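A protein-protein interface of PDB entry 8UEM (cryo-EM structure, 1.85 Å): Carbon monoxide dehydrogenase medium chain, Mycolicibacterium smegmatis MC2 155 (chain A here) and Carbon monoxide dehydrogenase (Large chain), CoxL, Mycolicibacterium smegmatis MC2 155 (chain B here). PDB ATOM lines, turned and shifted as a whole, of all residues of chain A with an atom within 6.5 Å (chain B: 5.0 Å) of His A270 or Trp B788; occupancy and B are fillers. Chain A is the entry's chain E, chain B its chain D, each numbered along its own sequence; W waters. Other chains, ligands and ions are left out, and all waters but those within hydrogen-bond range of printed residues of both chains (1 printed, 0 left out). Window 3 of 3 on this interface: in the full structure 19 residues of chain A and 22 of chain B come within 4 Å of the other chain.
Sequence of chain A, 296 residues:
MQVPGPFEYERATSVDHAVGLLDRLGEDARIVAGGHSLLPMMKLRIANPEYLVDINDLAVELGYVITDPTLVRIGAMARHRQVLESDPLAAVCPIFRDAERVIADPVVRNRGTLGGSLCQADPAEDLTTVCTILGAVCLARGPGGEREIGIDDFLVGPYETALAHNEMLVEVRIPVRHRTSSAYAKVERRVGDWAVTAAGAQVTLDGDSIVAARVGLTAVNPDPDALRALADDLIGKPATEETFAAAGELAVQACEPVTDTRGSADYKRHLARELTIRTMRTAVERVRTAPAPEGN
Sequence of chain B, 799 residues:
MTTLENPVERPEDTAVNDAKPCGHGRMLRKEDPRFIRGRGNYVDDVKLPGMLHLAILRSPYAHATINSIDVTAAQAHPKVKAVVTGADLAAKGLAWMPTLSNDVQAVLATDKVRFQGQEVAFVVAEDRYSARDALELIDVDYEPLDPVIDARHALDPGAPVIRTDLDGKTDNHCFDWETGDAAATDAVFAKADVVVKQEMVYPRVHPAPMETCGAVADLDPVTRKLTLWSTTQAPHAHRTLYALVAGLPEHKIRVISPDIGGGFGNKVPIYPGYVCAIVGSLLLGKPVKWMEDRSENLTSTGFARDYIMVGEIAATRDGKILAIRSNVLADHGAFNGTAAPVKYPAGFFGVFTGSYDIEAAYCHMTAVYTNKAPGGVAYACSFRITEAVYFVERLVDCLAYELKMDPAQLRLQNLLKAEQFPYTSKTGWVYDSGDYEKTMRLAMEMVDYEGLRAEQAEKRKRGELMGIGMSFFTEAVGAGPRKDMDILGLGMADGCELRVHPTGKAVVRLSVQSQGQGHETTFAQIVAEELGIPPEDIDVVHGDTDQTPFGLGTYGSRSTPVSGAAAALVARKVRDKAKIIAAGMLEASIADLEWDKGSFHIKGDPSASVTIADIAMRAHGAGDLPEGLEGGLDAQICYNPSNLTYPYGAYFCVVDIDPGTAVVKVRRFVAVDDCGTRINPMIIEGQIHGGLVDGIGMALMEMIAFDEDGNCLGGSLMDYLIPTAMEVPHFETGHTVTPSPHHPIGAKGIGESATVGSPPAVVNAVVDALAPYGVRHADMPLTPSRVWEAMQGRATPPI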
ATOM      1  N   VAL A 252       4.151  13.192 -17.792  1.00  0.00           N
ATOM      2  CA  VAL A 252       5.018  12.027 -17.649  1.00  0.00           C
ATOM      3  C   VAL A 252       5.485  11.914 -16.208  1.00  0.00           C
ATOM      4  O   VAL A 252       5.456  10.837 -15.601  1.00  0.00           O
ATOM      5  CB  VAL A 252       6.217  12.130 -18.608  1.00  0.00           C
ATOM      6  CG1 VAL A 252       7.297  11.128 -18.216  1.00  0.00           C
ATOM      7  CG2 VAL A 252       5.779  11.929 -20.036  1.00  0.00           C
ATOM      8  N   SER A 264       3.364  -1.606 -21.010  1.00  0.00           N
ATOM      9  CA  SER A 264       4.493  -1.317 -20.145  1.00  0.00           C
ATOM     10  C   SER A 264       4.323   0.038 -19.470  1.00  0.00           C
ATOM     11  O   SER A 264       3.670   0.944 -19.992  1.00  0.00           O
ATOM     12  CB  SER A 264       5.798  -1.346 -20.942  1.00  0.00           C
ATOM     13  OG  SER A 264       5.918  -0.213 -21.778  1.00  0.00           O
ATOM     14  N   ALA A 265       4.927   0.166 -18.289  1.00  0.00           N
ATOM     15  CA  ALA A 265       4.899   1.440 -17.584  1.00  0.00           C
ATOM     16  C   ALA A 265       5.528   2.540 -18.423  1.00  0.00           C
ATOM     17  O   ALA A 265       5.044   3.675 -18.432  1.00  0.00           O
ATOM     18  CB  ALA A 265       5.615   1.318 -16.243  1.00  0.00           C
ATOM     19  N   ASP A 266       6.615   2.223 -19.127  1.00  0.00           N
ATOM     20  CA  ASP A 266       7.233   3.208 -20.006  1.00  0.00           C
ATOM     21  C   ASP A 266       6.274   3.627 -21.109  1.00  0.00           C
ATOM     22  O   ASP A 266       6.202   4.808 -21.466  1.00  0.00           O
ATOM     23  CB  ASP A 266       8.526   2.652 -20.602  1.00  0.00           C
ATOM     24  CG  ASP A 266       9.584   2.382 -19.549  1.00  0.00           C
ATOM     25  OD1 ASP A 266       9.410   2.825 -18.396  1.00  0.00           O
ATOM     26  OD2 ASP A 266      10.592   1.722 -19.879  1.00  0.00           O
ATOM     27  N   TYR A 267       5.539   2.671 -21.675  1.00  0.00           N
ATOM     28  CA  TYR A 267       4.545   3.024 -22.680  1.00  0.00           C
ATOM     29  C   TYR A 267       3.435   3.867 -22.076  1.00  0.00           C
ATOM     30  O   TYR A 267       2.932   4.789 -22.719  1.00  0.00           O
ATOM     31  CB  TYR A 267       3.957   1.774 -23.321  1.00  0.00           C
ATOM     32  CG  TYR A 267       2.860   2.107 -24.296  1.00  0.00           C
ATOM     33  CD1 TYR A 267       3.140   2.790 -25.469  1.00  0.00           C
ATOM     34  CD2 TYR A 267       1.547   1.753 -24.040  1.00  0.00           C
ATOM     35  CE1 TYR A 267       2.142   3.102 -26.360  1.00  0.00           C
ATOM     36  CE2 TYR A 267       0.543   2.058 -24.928  1.00  0.00           C
ATOM     37  CZ  TYR A 267       0.842   2.739 -26.082  1.00  0.00           C
ATOM     38  OH  TYR A 267      -0.158   3.048 -26.964  1.00  0.00           O
ATOM     39  N   LYS A 268       3.032   3.558 -20.845  1.00  0.00           N
ATOM     40  CA  LYS A 268       2.021   4.367 -20.178  1.00  0.00           C
ATOM     41  C   LYS A 268       2.514   5.791 -19.970  1.00  0.00           C
ATOM     42  O   LYS A 268       1.740   6.739 -20.092  1.00  0.00           O
ATOM     43  CB  LYS A 268       1.641   3.739 -18.842  1.00  0.00           C
ATOM     44  CG  LYS A 268       1.301   2.272 -18.914  1.00  0.00           C
ATOM     45  CD  LYS A 268      -0.164   2.030 -19.077  1.00  0.00           C
ATOM     46  CE  LYS A 268      -0.460   0.548 -19.025  1.00  0.00           C
ATOM     47  NZ  LYS A 268      -0.436   0.044 -17.636  1.00  0.00           N
ATOM     48  N   ARG A 269       3.793   5.964 -19.636  1.00  0.00           N
ATOM     49  CA  ARG A 269       4.329   7.312 -19.460  1.00  0.00           C
ATOM     50  C   ARG A 269       4.411   8.044 -20.791  1.00  0.00           C
ATOM     51  O   ARG A 269       4.076   9.232 -20.884  1.00  0.00           O
ATOM     52  CB  ARG A 269       5.706   7.258 -18.799  1.00  0.00           C
ATOM     53  CG  ARG A 269       5.659   7.204 -17.286  1.00  0.00           C
ATOM     54  CD  ARG A 269       7.048   7.057 -16.698  1.00  0.00           C
ATOM     55  NE  ARG A 269       7.144   5.884 -15.841  1.00  0.00           N
ATOM     56  CZ  ARG A 269       7.814   4.784 -16.154  1.00  0.00           C
ATOM     57  NH1 ARG A 269       8.495   4.686 -17.284  1.00  0.00           N
ATOM     58  NH2 ARG A 269       7.799   3.755 -15.314  1.00  0.00           N
ATOM     59  N   HIS A 270       4.845   7.343 -21.835  1.00  0.00           N
ATOM     60  CA  HIS A 270       4.840   7.937 -23.160  1.00  0.00           C
ATOM     61  C   HIS A 270       3.433   8.358 -23.555  1.00  0.00           C
ATOM     62  O   HIS A 270       3.239   9.421 -24.146  1.00  0.00           O
ATOM     63  CB  HIS A 270       5.415   6.959 -24.180  1.00  0.00           C
ATOM     64  CG  HIS A 270       5.053   7.289 -25.589  1.00  0.00           C
ATOM     65  ND1 HIS A 270       5.743   8.219 -26.333  1.00  0.00           N
ATOM     66  CD2 HIS A 270       4.048   6.846 -26.378  1.00  0.00           C
ATOM     67  CE1 HIS A 270       5.191   8.321 -27.527  1.00  0.00           C
ATOM     68  NE2 HIS A 270       4.159   7.500 -27.580  1.00  0.00           N
ATOM     69  N   LEU A 271       2.439   7.530 -23.239  1.00  0.00           N
ATOM     70  CA  LEU A 271       1.054   7.879 -23.517  1.00  0.00           C
ATOM     71  C   LEU A 271       0.597   9.042 -22.653  1.00  0.00           C
ATOM     72  O   LEU A 271      -0.136   9.908 -23.120  1.00  0.00           O
ATOM     73  CB  LEU A 271       0.151   6.670 -23.296  1.00  0.00           C
ATOM     74  CG  LEU A 271       0.031   5.656 -24.430  1.00  0.00           C
ATOM     75  CD1 LEU A 271      -1.151   4.748 -24.164  1.00  0.00           C
ATOM     76  CD2 LEU A 271      -0.106   6.348 -25.773  1.00  0.00           C
ATOM     77  N   ALA A 272       1.000   9.075 -21.387  1.00  0.00           N
ATOM     78  CA  ALA A 272       0.671  10.224 -20.557  1.00  0.00           C
ATOM     79  C   ALA A 272       1.113  11.495 -21.255  1.00  0.00           C
ATOM     80  O   ALA A 272       0.317  12.413 -21.465  1.00  0.00           O
ATOM     81  CB  ALA A 272       1.323  10.092 -19.181  1.00  0.00           C
ATOM     82  N   ARG A 273       2.364  11.516 -21.717  1.00  0.00           N
ATOM     83  CA  ARG A 273       2.874  12.690 -22.418  1.00  0.00           C
ATOM     84  C   ARG A 273       2.105  12.954 -23.711  1.00  0.00           C
ATOM     85  O   ARG A 273       1.606  14.063 -23.937  1.00  0.00           O
ATOM     86  CB  ARG A 273       4.363  12.514 -22.710  1.00  0.00           C
ATOM     87  CG  ARG A 273       4.878  13.370 -23.842  1.00  0.00           C
ATOM     88  CD  ARG A 273       6.239  12.891 -24.328  1.00  0.00           C
ATOM     89  NE  ARG A 273       7.256  12.968 -23.288  1.00  0.00           N
ATOM     90  CZ  ARG A 273       7.907  11.923 -22.792  1.00  0.00           C
ATOM     91  NH1 ARG A 273       7.679  10.696 -23.228  1.00  0.00           N
ATOM     92  NH2 ARG A 273       8.810  12.117 -21.836  1.00  0.00           N
ATOM     93  N   GLU A 274       2.001  11.943 -24.575  1.00  0.00           N
ATOM     94  CA  GLU A 274       1.451  12.149 -25.911  1.00  0.00           C
ATOM     95  C   GLU A 274      -0.033  12.480 -25.855  1.00  0.00           C
ATOM     96  O   GLU A 274      -0.507  13.342 -26.593  1.00  0.00           O
ATOM     97  CB  GLU A 274       1.706  10.908 -26.769  1.00  0.00           C
ATOM     98  CG  GLU A 274       1.012  10.895 -28.123  1.00  0.00           C
ATOM     99  CD  GLU A 274       1.395  12.069 -29.005  1.00  0.00           C
ATOM    100  OE1 GLU A 274       2.479  12.651 -28.797  1.00  0.00           O
ATOM    101  OE2 GLU A 274       0.608  12.409 -29.912  1.00  0.00           O
ATOM    102  N   LEU A 275      -0.784  11.801 -24.990  1.00  0.00           N
ATOM    103  CA  LEU A 275      -2.204  12.078 -24.834  1.00  0.00           C
ATOM    104  C   LEU A 275      -2.438  13.408 -24.134  1.00  0.00           C
ATOM    105  O   LEU A 275      -3.391  14.115 -24.462  1.00  0.00           O
ATOM    106  CB  LEU A 275      -2.879  10.945 -24.069  1.00  0.00           C
ATOM    107  CG  LEU A 275      -2.811   9.563 -24.717  1.00  0.00           C
ATOM    108  CD1 LEU A 275      -3.610   8.576 -23.902  1.00  0.00           C
ATOM    109  CD2 LEU A 275      -3.310   9.610 -26.151  1.00  0.00           C
ATOM    110  N   GLY B 660       2.482   8.113 -32.743  1.00  0.00           N
ATOM    111  CA  GLY B 660       2.552   8.593 -31.379  1.00  0.00           C
ATOM    112  C   GLY B 660       2.109   7.565 -30.362  1.00  0.00           C
ATOM    113  O   GLY B 660       2.781   7.348 -29.353  1.00  0.00           O
ATOM    114  N   THR B 661       0.977   6.918 -30.625  1.00  0.00           N
ATOM    115  CA  THR B 661       0.395   5.958 -29.701  1.00  0.00           C
ATOM    116  C   THR B 661       0.701   4.513 -30.061  1.00  0.00           C
ATOM    117  O   THR B 661       0.385   3.618 -29.273  1.00  0.00           O
ATOM    118  CB  THR B 661      -1.125   6.148 -29.641  1.00  0.00           C
ATOM    119  OG1 THR B 661      -1.699   5.773 -30.895  1.00  0.00           O
ATOM    120  CG2 THR B 661      -1.467   7.603 -29.372  1.00  0.00           C
ATOM    121  N   ALA B 662       1.295   4.264 -31.228  1.00  0.00           N
ATOM    122  CA  ALA B 662       1.564   2.909 -31.702  1.00  0.00           C
ATOM    123  C   ALA B 662       0.290   2.077 -31.774  1.00  0.00           C
ATOM    124  O   ALA B 662       0.323   0.855 -31.632  1.00  0.00           O
ATOM    125  CB  ALA B 662       2.608   2.204 -30.832  1.00  0.00           C
ATOM    126  N   THR B 783      -0.095  -5.230 -29.541  1.00  0.00           N
ATOM    127  CA  THR B 783      -0.837  -4.237 -28.794  1.00  0.00           C
ATOM    128  C   THR B 783      -0.141  -2.890 -28.923  1.00  0.00           C
ATOM    129  O   THR B 783       1.012  -2.816 -29.350  1.00  0.00           O
ATOM    130  CB  THR B 783      -0.936  -4.632 -27.324  1.00  0.00           C
ATOM    131  OG1 THR B 783       0.364  -4.568 -26.731  1.00  0.00           O
ATOM    132  CG2 THR B 783      -1.476  -6.043 -27.188  1.00  0.00           C
ATOM    133  N   PRO B 784      -0.834  -1.802 -28.593  1.00  0.00           N
ATOM    134  CA  PRO B 784      -0.190  -0.484 -28.687  1.00  0.00           C
ATOM    135  C   PRO B 784       1.112  -0.412 -27.915  1.00  0.00           C
ATOM    136  O   PRO B 784       2.101   0.134 -28.419  1.00  0.00           O
ATOM    137  CB  PRO B 784      -1.256   0.457 -28.110  1.00  0.00           C
ATOM    138  CG  PRO B 784      -2.546  -0.254 -28.346  1.00  0.00           C
ATOM    139  CD  PRO B 784      -2.246  -1.707 -28.190  1.00  0.00           C
ATOM    140  N   SER B 785       1.145  -0.987 -26.711  1.00  0.00           N
ATOM    141  CA  SER B 785       2.354  -0.947 -25.899  1.00  0.00           C
ATOM    142  C   SER B 785       3.471  -1.762 -26.537  1.00  0.00           C
ATOM    143  O   SER B 785       4.618  -1.316 -26.597  1.00  0.00           O
ATOM    144  CB  SER B 785       2.057  -1.458 -24.489  1.00  0.00           C
ATOM    145  OG  SER B 785       3.213  -1.394 -23.676  1.00  0.00           O
ATOM    146  N   ARG B 786       3.156  -2.968 -27.005  1.00  0.00           N
ATOM    147  CA  ARG B 786       4.188  -3.829 -27.571  1.00  0.00           C
ATOM    148  C   ARG B 786       4.699  -3.275 -28.894  1.00  0.00           C
ATOM    149  O   ARG B 786       5.899  -3.335 -29.177  1.00  0.00           O
ATOM    150  CB  ARG B 786       3.649  -5.250 -27.717  1.00  0.00           C
ATOM    151  CG  ARG B 786       3.204  -5.857 -26.388  1.00  0.00           C
ATOM    152  CD  ARG B 786       2.766  -7.297 -26.547  1.00  0.00           C
ATOM    153  NE  ARG B 786       3.533  -7.942 -27.601  1.00  0.00           N
ATOM    154  CZ  ARG B 786       4.812  -8.266 -27.503  1.00  0.00           C
ATOM    155  NH1 ARG B 786       5.473  -8.125 -26.366  1.00  0.00           N
ATOM    156  NH2 ARG B 786       5.443  -8.738 -28.572  1.00  0.00           N
ATOM    157  N   VAL B 787       3.810  -2.693 -29.698  1.00  0.00           N
ATOM    158  CA  VAL B 787       4.244  -2.056 -30.934  1.00  0.00           C
ATOM    159  C   VAL B 787       5.123  -0.849 -30.634  1.00  0.00           C
ATOM    160  O   VAL B 787       6.128  -0.614 -31.310  1.00  0.00           O
ATOM    161  CB  VAL B 787       3.034  -1.660 -31.792  1.00  0.00           C
ATOM    162  CG1 VAL B 787       3.497  -0.839 -32.977  1.00  0.00           C
ATOM    163  CG2 VAL B 787       2.279  -2.890 -32.243  1.00  0.00           C
ATOM    164  N   TRP B 788       4.745  -0.052 -29.633  1.00  0.00           N
ATOM    165  CA  TRP B 788       5.562   1.095 -29.260  1.00  0.00           C
ATOM    166  C   TRP B 788       6.926   0.653 -28.754  1.00  0.00           C
ATOM    167  O   TRP B 788       7.946   1.260 -29.095  1.00  0.00           O
ATOM    168  CB  TRP B 788       4.845   1.924 -28.200  1.00  0.00           C
ATOM    169  CG  TRP B 788       5.661   3.065 -27.728  1.00  0.00           C
ATOM    170  CD1 TRP B 788       5.804   4.269 -28.334  1.00  0.00           C
ATOM    171  CD2 TRP B 788       6.464   3.108 -26.549  1.00  0.00           C
ATOM    172  NE1 TRP B 788       6.640   5.070 -27.605  1.00  0.00           N
ATOM    173  CE2 TRP B 788       7.061   4.380 -26.501  1.00  0.00           C
ATOM    174  CE3 TRP B 788       6.733   2.200 -25.526  1.00  0.00           C
ATOM    175  CZ2 TRP B 788       7.910   4.764 -25.475  1.00  0.00           C
ATOM    176  CZ3 TRP B 788       7.574   2.584 -24.509  1.00  0.00           C
ATOM    177  CH2 TRP B 788       8.155   3.853 -24.490  1.00  0.00           C
ATOM    178  N   GLU B 789       6.964  -0.405 -27.947  1.00  0.00           N
ATOM    179  CA  GLU B 789       8.239  -0.942 -27.487  1.00  0.00           C
ATOM    180  C   GLU B 789       9.089  -1.408 -28.659  1.00  0.00           C
ATOM    181  O   GLU B 789      10.303  -1.186 -28.680  1.00  0.00           O
ATOM    182  CB  GLU B 789       8.008  -2.089 -26.506  1.00  0.00           C
ATOM    183  CG  GLU B 789       7.265  -1.690 -25.241  1.00  0.00           C
ATOM    184  CD  GLU B 789       8.169  -1.018 -24.225  1.00  0.00           C
ATOM    185  OE1 GLU B 789       9.381  -1.321 -24.213  1.00  0.00           O
ATOM    186  OE2 GLU B 789       7.675  -0.178 -23.446  1.00  0.00           O
ATOM    187  N   ALA B 790       8.468  -2.055 -29.645  1.00  0.00           N
ATOM    188  CA  ALA B 790       9.189  -2.392 -30.865  1.00  0.00           C
ATOM    189  C   ALA B 790       9.722  -1.139 -31.544  1.00  0.00           C
ATOM    190  O   ALA B 790      10.844  -1.132 -32.058  1.00  0.00           O
ATOM    191  CB  ALA B 790       8.285  -3.179 -31.812  1.00  0.00           C
ATOM    192  N   MET B 791       8.933  -0.063 -31.550  1.00  0.00           N
ATOM    193  CA  MET B 791       9.407   1.195 -32.115  1.00  0.00           C
ATOM    194  C   MET B 791      10.647   1.685 -31.381  1.00  0.00           C
ATOM    195  O   MET B 791      11.587   2.190 -32.002  1.00  0.00           O
ATOM    196  CB  MET B 791       8.308   2.254 -32.046  1.00  0.00           C
ATOM    197  CG  MET B 791       7.029   1.903 -32.761  1.00  0.00           C
ATOM    198  SD  MET B 791       5.804   3.200 -32.492  1.00  0.00           S
ATOM    199  CE  MET B 791       4.919   3.165 -34.038  1.00  0.00           C
ATOM    200  N   GLN B 792      10.665   1.545 -30.056  1.00  0.00           N
ATOM    201  CA  GLN B 792      11.803   1.953 -29.242  1.00  0.00           C
ATOM    202  C   GLN B 792      13.017   1.068 -29.442  1.00  0.00           C
ATOM    203  O   GLN B 792      14.018   1.260 -28.748  1.00  0.00           O
ATOM    204  CB  GLN B 792      11.426   1.950 -27.760  1.00  0.00           C
ATOM    205  CG  GLN B 792      10.118   2.628 -27.435  1.00  0.00           C
ATOM    206  CD  GLN B 792       9.941   3.924 -28.181  1.00  0.00           C
ATOM    207  OE1 GLN B 792       9.045   4.056 -29.011  1.00  0.00           O
ATOM    208  NE2 GLN B 792      10.803   4.890 -27.900  1.00  0.00           N
ATOM    209  N   ARG B 794      13.011  -1.994 -28.593  1.00  0.00           N
ATOM    210  CA  ARG B 794      12.954  -2.932 -27.480  1.00  0.00           C
ATOM    211  C   ARG B 794      11.932  -4.039 -27.718  1.00  0.00           C
ATOM    212  O   ARG B 794      11.308  -4.526 -26.774  1.00  0.00           O
ATOM    213  CB  ARG B 794      12.641  -2.204 -26.175  1.00  0.00           C
ATOM    214  CG  ARG B 794      13.632  -1.116 -25.792  1.00  0.00           C
ATOM    215  CD  ARG B 794      13.434  -0.693 -24.342  1.00  0.00           C
ATOM    216  NE  ARG B 794      12.165  -0.006 -24.135  1.00  0.00           N
ATOM    217  CZ  ARG B 794      11.976   1.289 -24.341  1.00  0.00           C
ATOM    218  NH1 ARG B 794      12.957   2.072 -24.758  1.00  0.00           N
ATOM    219  NH2 ARG B 794      10.774   1.813 -24.125  1.00  0.00           N
HETATM  220  O   HOH W   1       5.425   7.464 -30.380  1.00  0.00           O
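The backbone carbonyl oxygen of Thr B661 sits at hydrogen-bond distance from the side-chain hydroxyl of Tyr A267 (2.4 Å).
The indole nitrogen (NE1) of Trp B788 sits close to a ring nitrogen (NE2) of His A270 (3.5 Å).
OG of Ser B785 sits at hydrogen-bond distance from N of Ser A264 (2.7 Å).
NE2 of His A270 sits close to O of Gly B660 (2.3 Å).
The side-chain hydroxyl of Ser A264 lies within hydrogen-bond range of the side-chain carboxylate of Glu B789 (2.4 Å).
Among the printed residues, pairs that only touch across the chains: Tyr A267 with Pro B784 (3.0 Å), Tyr A267 with Ser B785 (3.3 Å), Tyr A267 with Trp B788 (3.3 Å), Asp A266 with Trp B788 (3.7 Å), Tyr A267 with Glu B789 (3.98 Å) and Leu A271 with Thr B661 (3.98 Å).
His A270 touches two residues of chain B.
Trp B788 touches just these residues of chain A: Asp A266 (3.7 Å), Tyr A267 (3.3 Å) and His A270 (3.4 Å).
Printed residues of chain A within 4 Å of Ser B785: Ser A264 and Tyr A267.
Printed residues of chain B within 4 Å of Asp A266: Trp B788.
Of the printed residues of chain B, Tyr A267 touches Thr B661 (2.4 Å), Pro B784 (3.0 Å), Ser B785 (3.3 Å), Trp B788 (3.3 Å) and Glu B789 (3.98 Å).
Ala B662 touches none of the printed residues of chain A.
Arg A269 touches none of the printed residues of chain B.
The nearest residue of chain B that does not touch His A270 is Thr B661 (4.4 Å).
The nearest residue of chain A that does not touch Trp B788 is Ser A264 (4.2 Å).
The guanidinium group of Arg A269 lies within salt-bridge range of the side-chain carboxylate of Asp A266 (3.6 Å).
The indole nitrogen of Trp B788 lies within hydrogen-bond range of the side-chain amide oxygen of Gln B792, 3.0 Å away.
NE of Arg B794 lies within salt-bridge range of OE1 of Glu B789.
The side-chain hydroxyl (OG) of Ser A264 sits at hydrogen-bond distance from the backbone NH (N) of Tyr A267.
Printed residues of chain A that touch a printed residue of chain B: Ser A264, Asp A266, Tyr A267, His A270 and Leu A271.
Hydrophobic or aromatic side chains of chain A that line the printed part of chain B: Tyr A267, His A270 and Leu A271.
Of the 14 printed residues of chain B, 6 touch a printed residue of chain A.
Printed residues of chain B that touch a printed residue of chain A: Gly B660, Thr B661, Pro B784, Ser B785, Trp B788 and Glu B789.
Hydrophobic or aromatic side chains of chain B within 4 Å of the printed part of chain A: Pro B784 and Trp B788.
Along chain B the printed residues that touch a printed residue of chain A span positions 660 to 789.
Among the printed residues, no Asp or Glu carboxylate lies within 4 Å of a Lys or Arg side-chain nitrogen of the other chain.
Water W1 lies within hydrogen-bond range of O of Gly B660 (2.8 Å) and NE2 of His A270 (3.1 Å).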
